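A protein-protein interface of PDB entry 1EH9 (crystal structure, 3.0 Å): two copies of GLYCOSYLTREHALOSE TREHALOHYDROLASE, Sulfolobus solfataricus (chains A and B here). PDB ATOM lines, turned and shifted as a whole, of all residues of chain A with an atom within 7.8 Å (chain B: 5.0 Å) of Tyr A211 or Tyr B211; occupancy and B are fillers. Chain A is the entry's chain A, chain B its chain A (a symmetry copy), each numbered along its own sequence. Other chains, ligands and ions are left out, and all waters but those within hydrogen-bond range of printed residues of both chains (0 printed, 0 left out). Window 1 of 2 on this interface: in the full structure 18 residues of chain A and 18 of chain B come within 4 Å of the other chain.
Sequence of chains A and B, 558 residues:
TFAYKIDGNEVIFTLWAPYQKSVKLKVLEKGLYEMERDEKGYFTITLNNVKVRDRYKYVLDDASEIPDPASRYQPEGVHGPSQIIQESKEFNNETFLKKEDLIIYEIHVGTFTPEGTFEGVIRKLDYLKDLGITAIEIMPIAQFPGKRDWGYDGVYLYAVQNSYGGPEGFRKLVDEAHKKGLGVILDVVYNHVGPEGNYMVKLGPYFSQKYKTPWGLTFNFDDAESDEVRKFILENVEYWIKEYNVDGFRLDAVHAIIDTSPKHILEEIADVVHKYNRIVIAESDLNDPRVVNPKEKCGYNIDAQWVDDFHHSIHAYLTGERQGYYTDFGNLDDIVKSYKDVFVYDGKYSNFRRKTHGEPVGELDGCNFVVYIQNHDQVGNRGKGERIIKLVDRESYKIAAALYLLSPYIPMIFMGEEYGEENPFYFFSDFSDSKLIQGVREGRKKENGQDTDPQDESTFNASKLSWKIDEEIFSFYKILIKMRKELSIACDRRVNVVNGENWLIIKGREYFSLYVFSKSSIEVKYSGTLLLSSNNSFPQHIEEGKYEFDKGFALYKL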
ATOM      1  N   PHE A 207      -0.030  13.580  36.412  1.00  0.00           N
ATOM      2  CA  PHE A 207       0.210  13.256  35.006  1.00  0.00           C
ATOM      3  C   PHE A 207      -0.941  13.457  34.036  1.00  0.00           C
ATOM      4  O   PHE A 207      -2.091  13.104  34.298  1.00  0.00           O
ATOM      5  CB  PHE A 207       0.750  11.830  34.849  1.00  0.00           C
ATOM      6  CG  PHE A 207       1.613  11.474  36.022  1.00  0.00           C
ATOM      7  CD1 PHE A 207       1.094  10.728  37.082  1.00  0.00           C
ATOM      8  CD2 PHE A 207       2.933  11.927  36.088  1.00  0.00           C
ATOM      9  CE1 PHE A 207       1.877  10.418  38.191  1.00  0.00           C
ATOM     10  CE2 PHE A 207       3.736  11.629  37.186  1.00  0.00           C
ATOM     11  CZ  PHE A 207       3.195  10.879  38.232  1.00  0.00           C
ATOM     12  N   SER A 208      -0.578  13.951  32.860  1.00  0.00           N
ATOM     13  CA  SER A 208      -1.541  14.203  31.809  1.00  0.00           C
ATOM     14  C   SER A 208      -2.043  12.956  31.157  1.00  0.00           C
ATOM     15  O   SER A 208      -1.284  12.028  30.895  1.00  0.00           O
ATOM     16  CB  SER A 208      -1.108  15.227  30.775  1.00  0.00           C
ATOM     17  OG  SER A 208      -1.666  14.868  29.537  1.00  0.00           O
ATOM     18  N   GLN A 209      -3.344  12.982  30.890  1.00  0.00           N
ATOM     19  CA  GLN A 209      -4.050  11.876  30.275  1.00  0.00           C
ATOM     20  C   GLN A 209      -4.234  12.087  28.794  1.00  0.00           C
ATOM     21  O   GLN A 209      -4.455  11.135  28.040  1.00  0.00           O
ATOM     22  CB  GLN A 209      -5.405  11.684  30.930  1.00  0.00           C
ATOM     23  CG  GLN A 209      -5.933  13.028  31.449  1.00  0.00           C
ATOM     24  CD  GLN A 209      -7.018  12.833  32.477  1.00  0.00           C
ATOM     25  OE1 GLN A 209      -6.724  12.529  33.650  1.00  0.00           O
ATOM     26  NE2 GLN A 209      -8.275  12.952  32.022  1.00  0.00           N
ATOM     27  N   LYS A 210      -4.133  13.343  28.382  1.00  0.00           N
ATOM     28  CA  LYS A 210      -4.238  13.682  26.975  1.00  0.00           C
ATOM     29  C   LYS A 210      -3.190  12.928  26.166  1.00  0.00           C
ATOM     30  O   LYS A 210      -3.452  12.501  25.046  1.00  0.00           O
ATOM     31  CB  LYS A 210      -4.079  15.180  26.731  1.00  0.00           C
ATOM     32  CG  LYS A 210      -4.141  16.012  28.016  1.00  0.00           C
ATOM     33  CD  LYS A 210      -3.288  17.281  27.995  1.00  0.00           C
ATOM     34  CE  LYS A 210      -3.835  18.379  27.086  1.00  0.00           C
ATOM     35  NZ  LYS A 210      -3.158  19.673  27.279  1.00  0.00           N
ATOM     36  N   TYR A 211      -1.995  12.765  26.739  1.00  0.00           N
ATOM     37  CA  TYR A 211      -0.941  12.072  26.035  1.00  0.00           C
ATOM     38  C   TYR A 211      -0.361  10.814  26.683  1.00  0.00           C
ATOM     39  O   TYR A 211      -0.523  10.542  27.891  1.00  0.00           O
ATOM     40  CB  TYR A 211       0.222  12.988  25.728  1.00  0.00           C
ATOM     41  CG  TYR A 211      -0.051  14.441  25.834  1.00  0.00           C
ATOM     42  CD1 TYR A 211      -0.630  15.113  24.762  1.00  0.00           C
ATOM     43  CD2 TYR A 211       0.382  15.171  26.940  1.00  0.00           C
ATOM     44  CE1 TYR A 211      -0.820  16.493  24.802  1.00  0.00           C
ATOM     45  CE2 TYR A 211       0.198  16.553  27.003  1.00  0.00           C
ATOM     46  CZ  TYR A 211      -0.408  17.206  25.924  1.00  0.00           C
ATOM     47  OH  TYR A 211      -0.621  18.547  25.924  1.00  0.00           O
ATOM     48  N   LYS A 212       0.392  10.093  25.821  1.00  0.00           N
ATOM     49  CA  LYS A 212       1.097   8.867  26.162  1.00  0.00           C
ATOM     50  C   LYS A 212       2.482   8.713  25.480  1.00  0.00           C
ATOM     51  O   LYS A 212       2.587   8.469  24.272  1.00  0.00           O
ATOM     52  CB  LYS A 212       0.214   7.628  26.045  1.00  0.00           C
ATOM     53  CG  LYS A 212      -0.112   7.255  24.608  1.00  0.00           C
ATOM     54  CD  LYS A 212      -1.599   7.011  24.364  1.00  0.00           C
ATOM     55  CE  LYS A 212      -1.872   6.077  23.183  1.00  0.00           C
ATOM     56  NZ  LYS A 212      -0.752   6.002  22.220  1.00  0.00           N
ATOM     57  N   THR A 213       3.548   8.882  26.300  1.00  0.00           N
ATOM     58  CA  THR A 213       4.952   8.751  25.891  1.00  0.00           C
ATOM     59  C   THR A 213       5.191   7.263  25.554  1.00  0.00           C
ATOM     60  O   THR A 213       4.322   6.657  24.909  1.00  0.00           O
ATOM     61  CB  THR A 213       5.937   9.369  26.956  1.00  0.00           C
ATOM     62  OG1 THR A 213       5.851   8.777  28.259  1.00  0.00           O
ATOM     63  CG2 THR A 213       5.871  10.898  27.014  1.00  0.00           C
ATOM     64  N   GLY A 216       4.885   4.970  29.567  1.00  0.00           N
ATOM     65  CA  GLY A 216       3.629   5.395  30.116  1.00  0.00           C
ATOM     66  C   GLY A 216       3.317   6.812  29.692  1.00  0.00           C
ATOM     67  O   GLY A 216       3.187   7.104  28.503  1.00  0.00           O
ATOM     68  N   LEU A 217       3.245   7.693  30.686  1.00  0.00           N
ATOM     69  CA  LEU A 217       2.893   9.071  30.440  1.00  0.00           C
ATOM     70  C   LEU A 217       3.701  10.111  31.195  1.00  0.00           C
ATOM     71  O   LEU A 217       4.199   9.880  32.299  1.00  0.00           O
ATOM     72  CB  LEU A 217       1.392   9.272  30.720  1.00  0.00           C
ATOM     73  CG  LEU A 217       0.715   7.972  31.172  1.00  0.00           C
ATOM     74  CD1 LEU A 217       1.189   7.564  32.577  1.00  0.00           C
ATOM     75  CD2 LEU A 217      -0.810   8.127  31.118  1.00  0.00           C
ATOM     76  N   THR A 218       3.784  11.279  30.559  1.00  0.00           N
ATOM     77  CA  THR A 218       4.461  12.431  31.078  1.00  0.00           C
ATOM     78  C   THR A 218       3.518  13.048  32.101  1.00  0.00           C
ATOM     79  O   THR A 218       2.457  12.499  32.375  1.00  0.00           O
ATOM     80  CB  THR A 218       4.876  13.376  29.895  1.00  0.00           C
ATOM     81  OG1 THR A 218       5.329  14.666  30.277  1.00  0.00           O
ATOM     82  CG2 THR A 218       3.749  13.503  28.887  1.00  0.00           C
ATOM     83  N   PHE A 219       3.932  14.148  32.685  1.00  0.00           N
ATOM     84  CA  PHE A 219       3.146  14.845  33.642  1.00  0.00           C
ATOM     85  C   PHE A 219       2.171  15.768  32.961  1.00  0.00           C
ATOM     86  O   PHE A 219       2.130  15.890  31.722  1.00  0.00           O
ATOM     87  CB  PHE A 219       4.026  15.808  34.379  1.00  0.00           C
ATOM     88  CG  PHE A 219       5.038  15.173  35.230  1.00  0.00           C
ATOM     89  CD1 PHE A 219       4.688  14.605  36.454  1.00  0.00           C
ATOM     90  CD2 PHE A 219       6.372  15.231  34.842  1.00  0.00           C
ATOM     91  CE1 PHE A 219       5.663  14.066  37.286  1.00  0.00           C
ATOM     92  CE2 PHE A 219       7.361  14.691  35.659  1.00  0.00           C
ATOM     93  CZ  PHE A 219       6.995  14.119  36.877  1.00  0.00           C
ATOM     94  N   ASN A 220       1.475  16.514  33.822  1.00  0.00           N
ATOM     95  CA  ASN A 220       0.496  17.466  33.386  1.00  0.00           C
ATOM     96  C   ASN A 220       0.977  18.878  33.398  1.00  0.00           C
ATOM     97  O   ASN A 220       0.819  19.549  34.405  1.00  0.00           O
ATOM     98  CB  ASN A 220      -0.712  17.395  34.301  1.00  0.00           C
ATOM     99  CG  ASN A 220      -1.824  18.146  33.661  1.00  0.00           C
ATOM    100  OD1 ASN A 220      -1.927  18.148  32.416  1.00  0.00           O
ATOM    101  ND2 ASN A 220      -2.525  18.921  34.470  1.00  0.00           N
ATOM    102  N   PHE A 221       1.500  19.349  32.279  1.00  0.00           N
ATOM    103  CA  PHE A 221       2.015  20.725  32.226  1.00  0.00           C
ATOM    104  C   PHE A 221       1.065  21.694  31.584  1.00  0.00           C
ATOM    105  O   PHE A 221       1.337  22.895  31.558  1.00  0.00           O
ATOM    106  CB  PHE A 221       3.290  20.734  31.369  1.00  0.00           C
ATOM    107  CG  PHE A 221       4.207  19.634  31.827  1.00  0.00           C
ATOM    108  CD1 PHE A 221       3.966  18.315  31.438  1.00  0.00           C
ATOM    109  CD2 PHE A 221       5.260  19.915  32.701  1.00  0.00           C
ATOM    110  CE1 PHE A 221       4.791  17.285  31.889  1.00  0.00           C
ATOM    111  CE2 PHE A 221       6.087  18.903  33.171  1.00  0.00           C
ATOM    112  CZ  PHE A 221       5.831  17.591  32.766  1.00  0.00           C
ATOM    113  N   ASP A 222      -0.022  21.095  31.054  1.00  0.00           N
ATOM    114  CA  ASP A 222      -1.069  21.665  30.218  1.00  0.00           C
ATOM    115  C   ASP A 222      -2.455  21.916  30.820  1.00  0.00           C
ATOM    116  O   ASP A 222      -2.786  23.033  31.196  1.00  0.00           O
ATOM    117  CB  ASP A 222      -1.184  20.729  29.003  1.00  0.00           C
ATOM    118  CG  ASP A 222      -0.265  21.228  27.959  1.00  0.00           C
ATOM    119  OD1 ASP A 222       0.501  22.169  28.146  1.00  0.00           O
ATOM    120  OD2 ASP A 222      -0.445  20.646  26.815  1.00  0.00           O
ATOM    121  N   ASP A 223      -3.286  20.870  30.824  1.00  0.00           N
ATOM    122  CA  ASP A 223      -4.676  20.893  31.284  1.00  0.00           C
ATOM    123  C   ASP A 223      -4.858  21.235  32.758  1.00  0.00           C
ATOM    124  O   ASP A 223      -4.081  21.955  33.369  1.00  0.00           O
ATOM    125  CB  ASP A 223      -5.337  19.507  31.032  1.00  0.00           C
ATOM    126  CG  ASP A 223      -6.421  19.434  29.979  1.00  0.00           C
ATOM    127  OD1 ASP A 223      -6.675  20.330  29.169  1.00  0.00           O
ATOM    128  OD2 ASP A 223      -7.035  18.264  30.007  1.00  0.00           O
ATOM    129  N   ALA A 256       9.723  13.929  25.520  1.00  0.00           N
ATOM    130  CA  ALA A 256       8.654  13.145  26.079  1.00  0.00           C
ATOM    131  C   ALA A 256       7.941  14.061  27.027  1.00  0.00           C
ATOM    132  O   ALA A 256       7.064  13.668  27.799  1.00  0.00           O
ATOM    133  CB  ALA A 256       9.180  11.932  26.801  1.00  0.00           C
ATOM    134  N   ILE A 257       8.382  15.313  26.930  1.00  0.00           N
ATOM    135  CA  ILE A 257       7.854  16.391  27.694  1.00  0.00           C
ATOM    136  C   ILE A 257       6.986  17.218  26.810  1.00  0.00           C
ATOM    137  O   ILE A 257       7.517  17.945  25.968  1.00  0.00           O
ATOM    138  CB  ILE A 257       8.930  17.304  28.175  1.00  0.00           C
ATOM    139  CG1 ILE A 257       9.587  16.701  29.397  1.00  0.00           C
ATOM    140  CG2 ILE A 257       8.323  18.653  28.544  1.00  0.00           C
ATOM    141  CD1 ILE A 257      10.767  17.553  29.834  1.00  0.00           C
ATOM    142  N   ILE A 258       5.655  17.083  27.019  1.00  0.00           N
ATOM    143  CA  ILE A 258       4.651  17.819  26.260  1.00  0.00           C
ATOM    144  C   ILE A 258       3.944  18.926  26.982  1.00  0.00           C
ATOM    145  O   ILE A 258       3.271  18.750  28.028  1.00  0.00           O
ATOM    146  CB  ILE A 258       3.759  17.018  25.407  1.00  0.00           C
ATOM    147  CG1 ILE A 258       4.224  15.568  25.464  1.00  0.00           C
ATOM    148  CG2 ILE A 258       3.982  17.608  24.048  1.00  0.00           C
ATOM    149  CD1 ILE A 258       4.571  14.962  24.102  1.00  0.00           C
ATOM    150  N   ASP A 259       4.156  20.075  26.378  1.00  0.00           N
ATOM    151  CA  ASP A 259       3.697  21.320  26.879  1.00  0.00           C
ATOM    152  C   ASP A 259       3.199  22.127  25.754  1.00  0.00           C
ATOM    153  O   ASP A 259       3.870  22.241  24.732  1.00  0.00           O
ATOM    154  CB  ASP A 259       4.894  22.070  27.404  1.00  0.00           C
ATOM    155  CG  ASP A 259       4.438  22.937  28.476  1.00  0.00           C
ATOM    156  OD1 ASP A 259       3.473  22.599  29.132  1.00  0.00           O
ATOM    157  OD2 ASP A 259       5.142  24.062  28.586  1.00  0.00           O
ATOM    158  N   THR A 260       2.031  22.703  25.933  1.00  0.00           N
ATOM    159  CA  THR A 260       1.452  23.489  24.852  1.00  0.00           C
ATOM    160  C   THR A 260       1.341  24.931  25.239  1.00  0.00           C
ATOM    161  O   THR A 260       1.065  25.782  24.379  1.00  0.00           O
ATOM    162  CB  THR A 260       0.058  22.975  24.463  1.00  0.00           C
ATOM    163  OG1 THR A 260      -0.789  23.225  25.544  1.00  0.00           O
ATOM    164  CG2 THR A 260       0.051  21.469  24.196  1.00  0.00           C
ATOM    165  N   SER A 261       1.549  25.157  26.552  1.00  0.00           N
ATOM    166  CA  SER A 261       1.458  26.467  27.163  1.00  0.00           C
ATOM    167  C   SER A 261       2.209  27.536  26.387  1.00  0.00           C
ATOM    168  O   SER A 261       3.026  27.212  25.547  1.00  0.00           O
ATOM    169  CB  SER A 261       1.784  26.377  28.623  1.00  0.00           C
ATOM    170  OG  SER A 261       1.136  25.224  29.184  1.00  0.00           O
ATOM    171  N   SER B 208      -3.195  10.282  14.665  1.00  0.00           N
ATOM    172  CA  SER B 208      -2.244  10.009  15.722  1.00  0.00           C
ATOM    173  C   SER B 208      -2.860   9.359  16.919  1.00  0.00           C
ATOM    174  O   SER B 208      -3.954   9.720  17.343  1.00  0.00           O
ATOM    175  CB  SER B 208      -1.377  11.189  16.126  1.00  0.00           C
ATOM    176  OG  SER B 208      -1.094  11.081  17.496  1.00  0.00           O
ATOM    177  N   GLN B 209      -2.108   8.403  17.452  1.00  0.00           N
ATOM    178  CA  GLN B 209      -2.513   7.627  18.606  1.00  0.00           C
ATOM    179  C   GLN B 209      -1.894   8.152  19.876  1.00  0.00           C
ATOM    180  O   GLN B 209      -2.388   7.892  20.976  1.00  0.00           O
ATOM    181  CB  GLN B 209      -2.130   6.170  18.423  1.00  0.00           C
ATOM    182  CG  GLN B 209      -0.872   6.062  17.550  1.00  0.00           C
ATOM    183  CD  GLN B 209      -0.719   4.677  16.975  1.00  0.00           C
ATOM    184  OE1 GLN B 209      -1.398   4.329  15.988  1.00  0.00           O
ATOM    185  NE2 GLN B 209       0.132   3.869  17.626  1.00  0.00           N
ATOM    186  N   LYS B 210      -0.812   8.901  19.713  1.00  0.00           N
ATOM    187  CA  LYS B 210      -0.146   9.513  20.847  1.00  0.00           C
ATOM    188  C   LYS B 210      -1.115  10.401  21.619  1.00  0.00           C
ATOM    189  O   LYS B 210      -1.068  10.464  22.842  1.00  0.00           O
ATOM    190  CB  LYS B 210       1.066  10.340  20.426  1.00  0.00           C
ATOM    191  CG  LYS B 210       1.479  10.104  18.970  1.00  0.00           C
ATOM    192  CD  LYS B 210       2.094  11.323  18.278  1.00  0.00           C
ATOM    193  CE  LYS B 210       3.496  11.674  18.772  1.00  0.00           C
ATOM    194  NZ  LYS B 210       4.170  12.671  17.923  1.00  0.00           N
ATOM    195  N   TYR B 211      -1.999  11.093  20.894  1.00  0.00           N
ATOM    196  CA  TYR B 211      -2.945  11.968  21.546  1.00  0.00           C
ATOM    197  C   TYR B 211      -4.434  11.686  21.338  1.00  0.00           C
ATOM    198  O   TYR B 211      -4.861  10.958  20.417  1.00  0.00           O
ATOM    199  CB  TYR B 211      -2.715  13.415  21.175  1.00  0.00           C
ATOM    200  CG  TYR B 211      -1.400  13.727  20.565  1.00  0.00           C
ATOM    201  CD1 TYR B 211      -0.295  13.947  21.381  1.00  0.00           C
ATOM    202  CD2 TYR B 211      -1.282  13.932  19.190  1.00  0.00           C
ATOM    203  CE1 TYR B 211       0.931  14.324  20.837  1.00  0.00           C
ATOM    204  CE2 TYR B 211      -0.062  14.306  18.625  1.00  0.00           C
ATOM    205  CZ  TYR B 211       1.043  14.499  19.461  1.00  0.00           C
ATOM    206  OH  TYR B 211       2.258  14.857  18.973  1.00  0.00           O
ATOM    207  N   LYS B 212      -5.212  12.364  22.212  1.00  0.00           N
ATOM    208  CA  LYS B 212      -6.665  12.321  22.235  1.00  0.00           C
ATOM    209  C   LYS B 212      -7.342  13.674  22.574  1.00  0.00           C
ATOM    210  O   LYS B 212      -7.312  14.149  23.715  1.00  0.00           O
ATOM    211  CB  LYS B 212      -7.206  11.145  23.044  1.00  0.00           C
ATOM    212  CG  LYS B 212      -7.008  11.303  24.543  1.00  0.00           C
ATOM    213  CD  LYS B 212      -6.387  10.077  25.208  1.00  0.00           C
ATOM    214  CE  LYS B 212      -6.738   9.953  26.692  1.00  0.00           C
ATOM    215  NZ  LYS B 212      -7.148  11.233  27.310  1.00  0.00           N
ATOM    216  N   THR B 213      -7.944  14.293  21.529  1.00  0.00           N
ATOM    217  CA  THR B 213      -8.676  15.564  21.611  1.00  0.00           C
ATOM    218  C   THR B 213      -9.947  15.302  22.449  1.00  0.00           C
ATOM    219  O   THR B 213      -9.848  14.602  23.468  1.00  0.00           O
ATOM    220  CB  THR B 213      -8.924  16.195  20.187  1.00  0.00           C
ATOM    221  OG1 THR B 213      -9.676  15.367  19.292  1.00  0.00           O
ATOM    222  CG2 THR B 213      -7.642  16.727  19.540  1.00  0.00           C
ATOM    223  N   LEU B 217      -9.806  11.812  18.194  1.00  0.00           N
ATOM    224  CA  LEU B 217      -8.430  12.169  17.943  1.00  0.00           C
ATOM    225  C   LEU B 217      -8.166  12.948  16.666  1.00  0.00           C
ATOM    226  O   LEU B 217      -8.872  12.825  15.664  1.00  0.00           O
ATOM    227  CB  LEU B 217      -7.559  10.899  17.969  1.00  0.00           C
ATOM    228  CG  LEU B 217      -8.391   9.642  18.249  1.00  0.00           C
ATOM    229  CD1 LEU B 217      -9.304   9.306  17.058  1.00  0.00           C
ATOM    230  CD2 LEU B 217      -7.468   8.467  18.596  1.00  0.00           C
ATOM    231  N   THR B 218      -7.095  13.737  16.742  1.00  0.00           N
ATOM    232  CA  THR B 218      -6.614  14.547  15.660  1.00  0.00           C
ATOM    233  C   THR B 218      -5.863  13.605  14.732  1.00  0.00           C
ATOM    234  O   THR B 218      -5.836  12.400  14.959  1.00  0.00           O
ATOM    235  CB  THR B 218      -5.767  15.740  16.231  1.00  0.00           C
ATOM    236  OG1 THR B 218      -5.026  16.475  15.270  1.00  0.00           O
ATOM    237  CG2 THR B 218      -4.847  15.266  17.339  1.00  0.00           C
ATOM    238  N   ASP B 222       2.841  14.313  13.270  1.00  0.00           N
ATOM    239  CA  ASP B 222       4.046  14.010  14.029  1.00  0.00           C
ATOM    240  C   ASP B 222       4.822  12.725  13.724  1.00  0.00           C
ATOM    241  O   ASP B 222       5.825  12.748  13.021  1.00  0.00           O
ATOM    242  CB  ASP B 222       3.620  14.029  15.508  1.00  0.00           C
ATOM    243  CG  ASP B 222       3.806  15.404  16.014  1.00  0.00           C
ATOM    244  OD1 ASP B 222       4.146  16.337  15.291  1.00  0.00           O
ATOM    245  OD2 ASP B 222       3.689  15.483  17.304  1.00  0.00           O
ATOM    246  N   ILE B 258      -2.430  19.012  17.108  1.00  0.00           N
ATOM    247  CA  ILE B 258      -1.128  18.782  17.723  1.00  0.00           C
ATOM    248  C   ILE B 258      -0.022  18.351  16.807  1.00  0.00           C
ATOM    249  O   ILE B 258      -0.070  17.306  16.110  1.00  0.00           O
ATOM    250  CB  ILE B 258      -1.129  18.068  19.010  1.00  0.00           C
ATOM    251  CG1 ILE B 258      -2.578  17.851  19.430  1.00  0.00           C
ATOM    252  CG2 ILE B 258      -0.436  19.032  19.923  1.00  0.00           C
ATOM    253  CD1 ILE B 258      -2.934  18.441  20.796  1.00  0.00           C
ATOM    254  N   THR B 260       4.323  18.698  16.674  1.00  0.00           N
ATOM    255  CA  THR B 260       5.525  18.968  17.453  1.00  0.00           C
ATOM    256  C   THR B 260       6.679  19.295  16.559  1.00  0.00           C
ATOM    257  O   THR B 260       7.727  19.752  17.044  1.00  0.00           O
ATOM    258  CB  THR B 260       5.908  17.769  18.333  1.00  0.00           C
ATOM    259  OG1 THR B 260       6.294  16.736  17.476  1.00  0.00           O
ATOM    260  CG2 THR B 260       4.732  17.269  19.173  1.00  0.00           C
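The backbone carbonyl oxygen (O) of Gln A209 lies within hydrogen-bond range of the side-chain amino group (NZ) of Lys B212 (2.8 Å). The backbone carbonyl oxygen of Lys A210 lies within hydrogen-bond range of the backbone NH of Lys B212 (3.3 Å). The side-chain amino group (NZ) of Lys A212 lies within hydrogen-bond range of the backbone carbonyl oxygen (O) of Gln B209 (2.8 Å). The backbone NH (N) of Lys A212 lies within hydrogen-bond range of the backbone carbonyl oxygen (O) of Lys B210 (3.3 Å).
OG of Ser A208 lies within hydrogen-bond range of N of Lys A210. OH of Tyr A211 is in hydrogen-bond range of NZ of Lys A210, 3.1 Å away. The side-chain amino group (NZ) of Lys A210 lies within salt-bridge range of the side-chain carboxylate (OD2) of Asp A222 (2.9 Å). OG of Ser B208 sits close to N of Lys B210. The side-chain amino group (NZ) of Lys B210 is in hydrogen-bond range of the side-chain hydroxyl (OH) of Tyr B211 (3.1 Å). The side-chain amino group of Lys B210 is in salt-bridge range of the side-chain carboxylate of Asp B222 (2.9 Å).
Among the printed residues, pairs that only touch across the chains: Lys A210 with Tyr B211, Tyr A211 with Lys B210, Tyr A211 with Tyr B211 and Lys A210 with Lys B210.
Of the printed residues of chain B, Gln A209 touches Lys B212. Tyr A211 touches two residues of chain B. Asp A223 touches none of the printed residues of chain B. Asp A259 touches none of the printed residues of chain B. Of the printed residues of chain A, Gln B209 touches Lys A212. The nearest residue of chain A that does not touch Tyr B211 is Ile A258 (4.9 Å). The nearest printed residue of chain A that does not touch Lys B212 is Tyr A211 (5.4 Å).
Hydrophobic or aromatic side chains of chain B that line the printed part of chain A: Tyr B211. Hydrophobic or aromatic side chains of chain A within 4 Å of the printed part of chain B: Tyr A211. Among the printed residues, 8 pairs touch across the chains. Among the printed residues, no Asp or Glu carboxylate lies within 4 Å of a Lys or Arg side-chain nitrogen of the other chain.
Gln A209 touches Lys B212, and with the chains exchanged Lys A212 touches Gln B209. Lys B210 touches its own counterpart, Lys A210. Lys A210 touches Tyr B211, and with the chains exchanged Tyr A211 touches Lys B210. Lys A210 touches Lys B212, and with the chains exchanged Lys A212 touches Lys B210. Of the 8 pairs that touch across the chains among the printed residues, 8 have their exchanged pair printed and touching as well.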
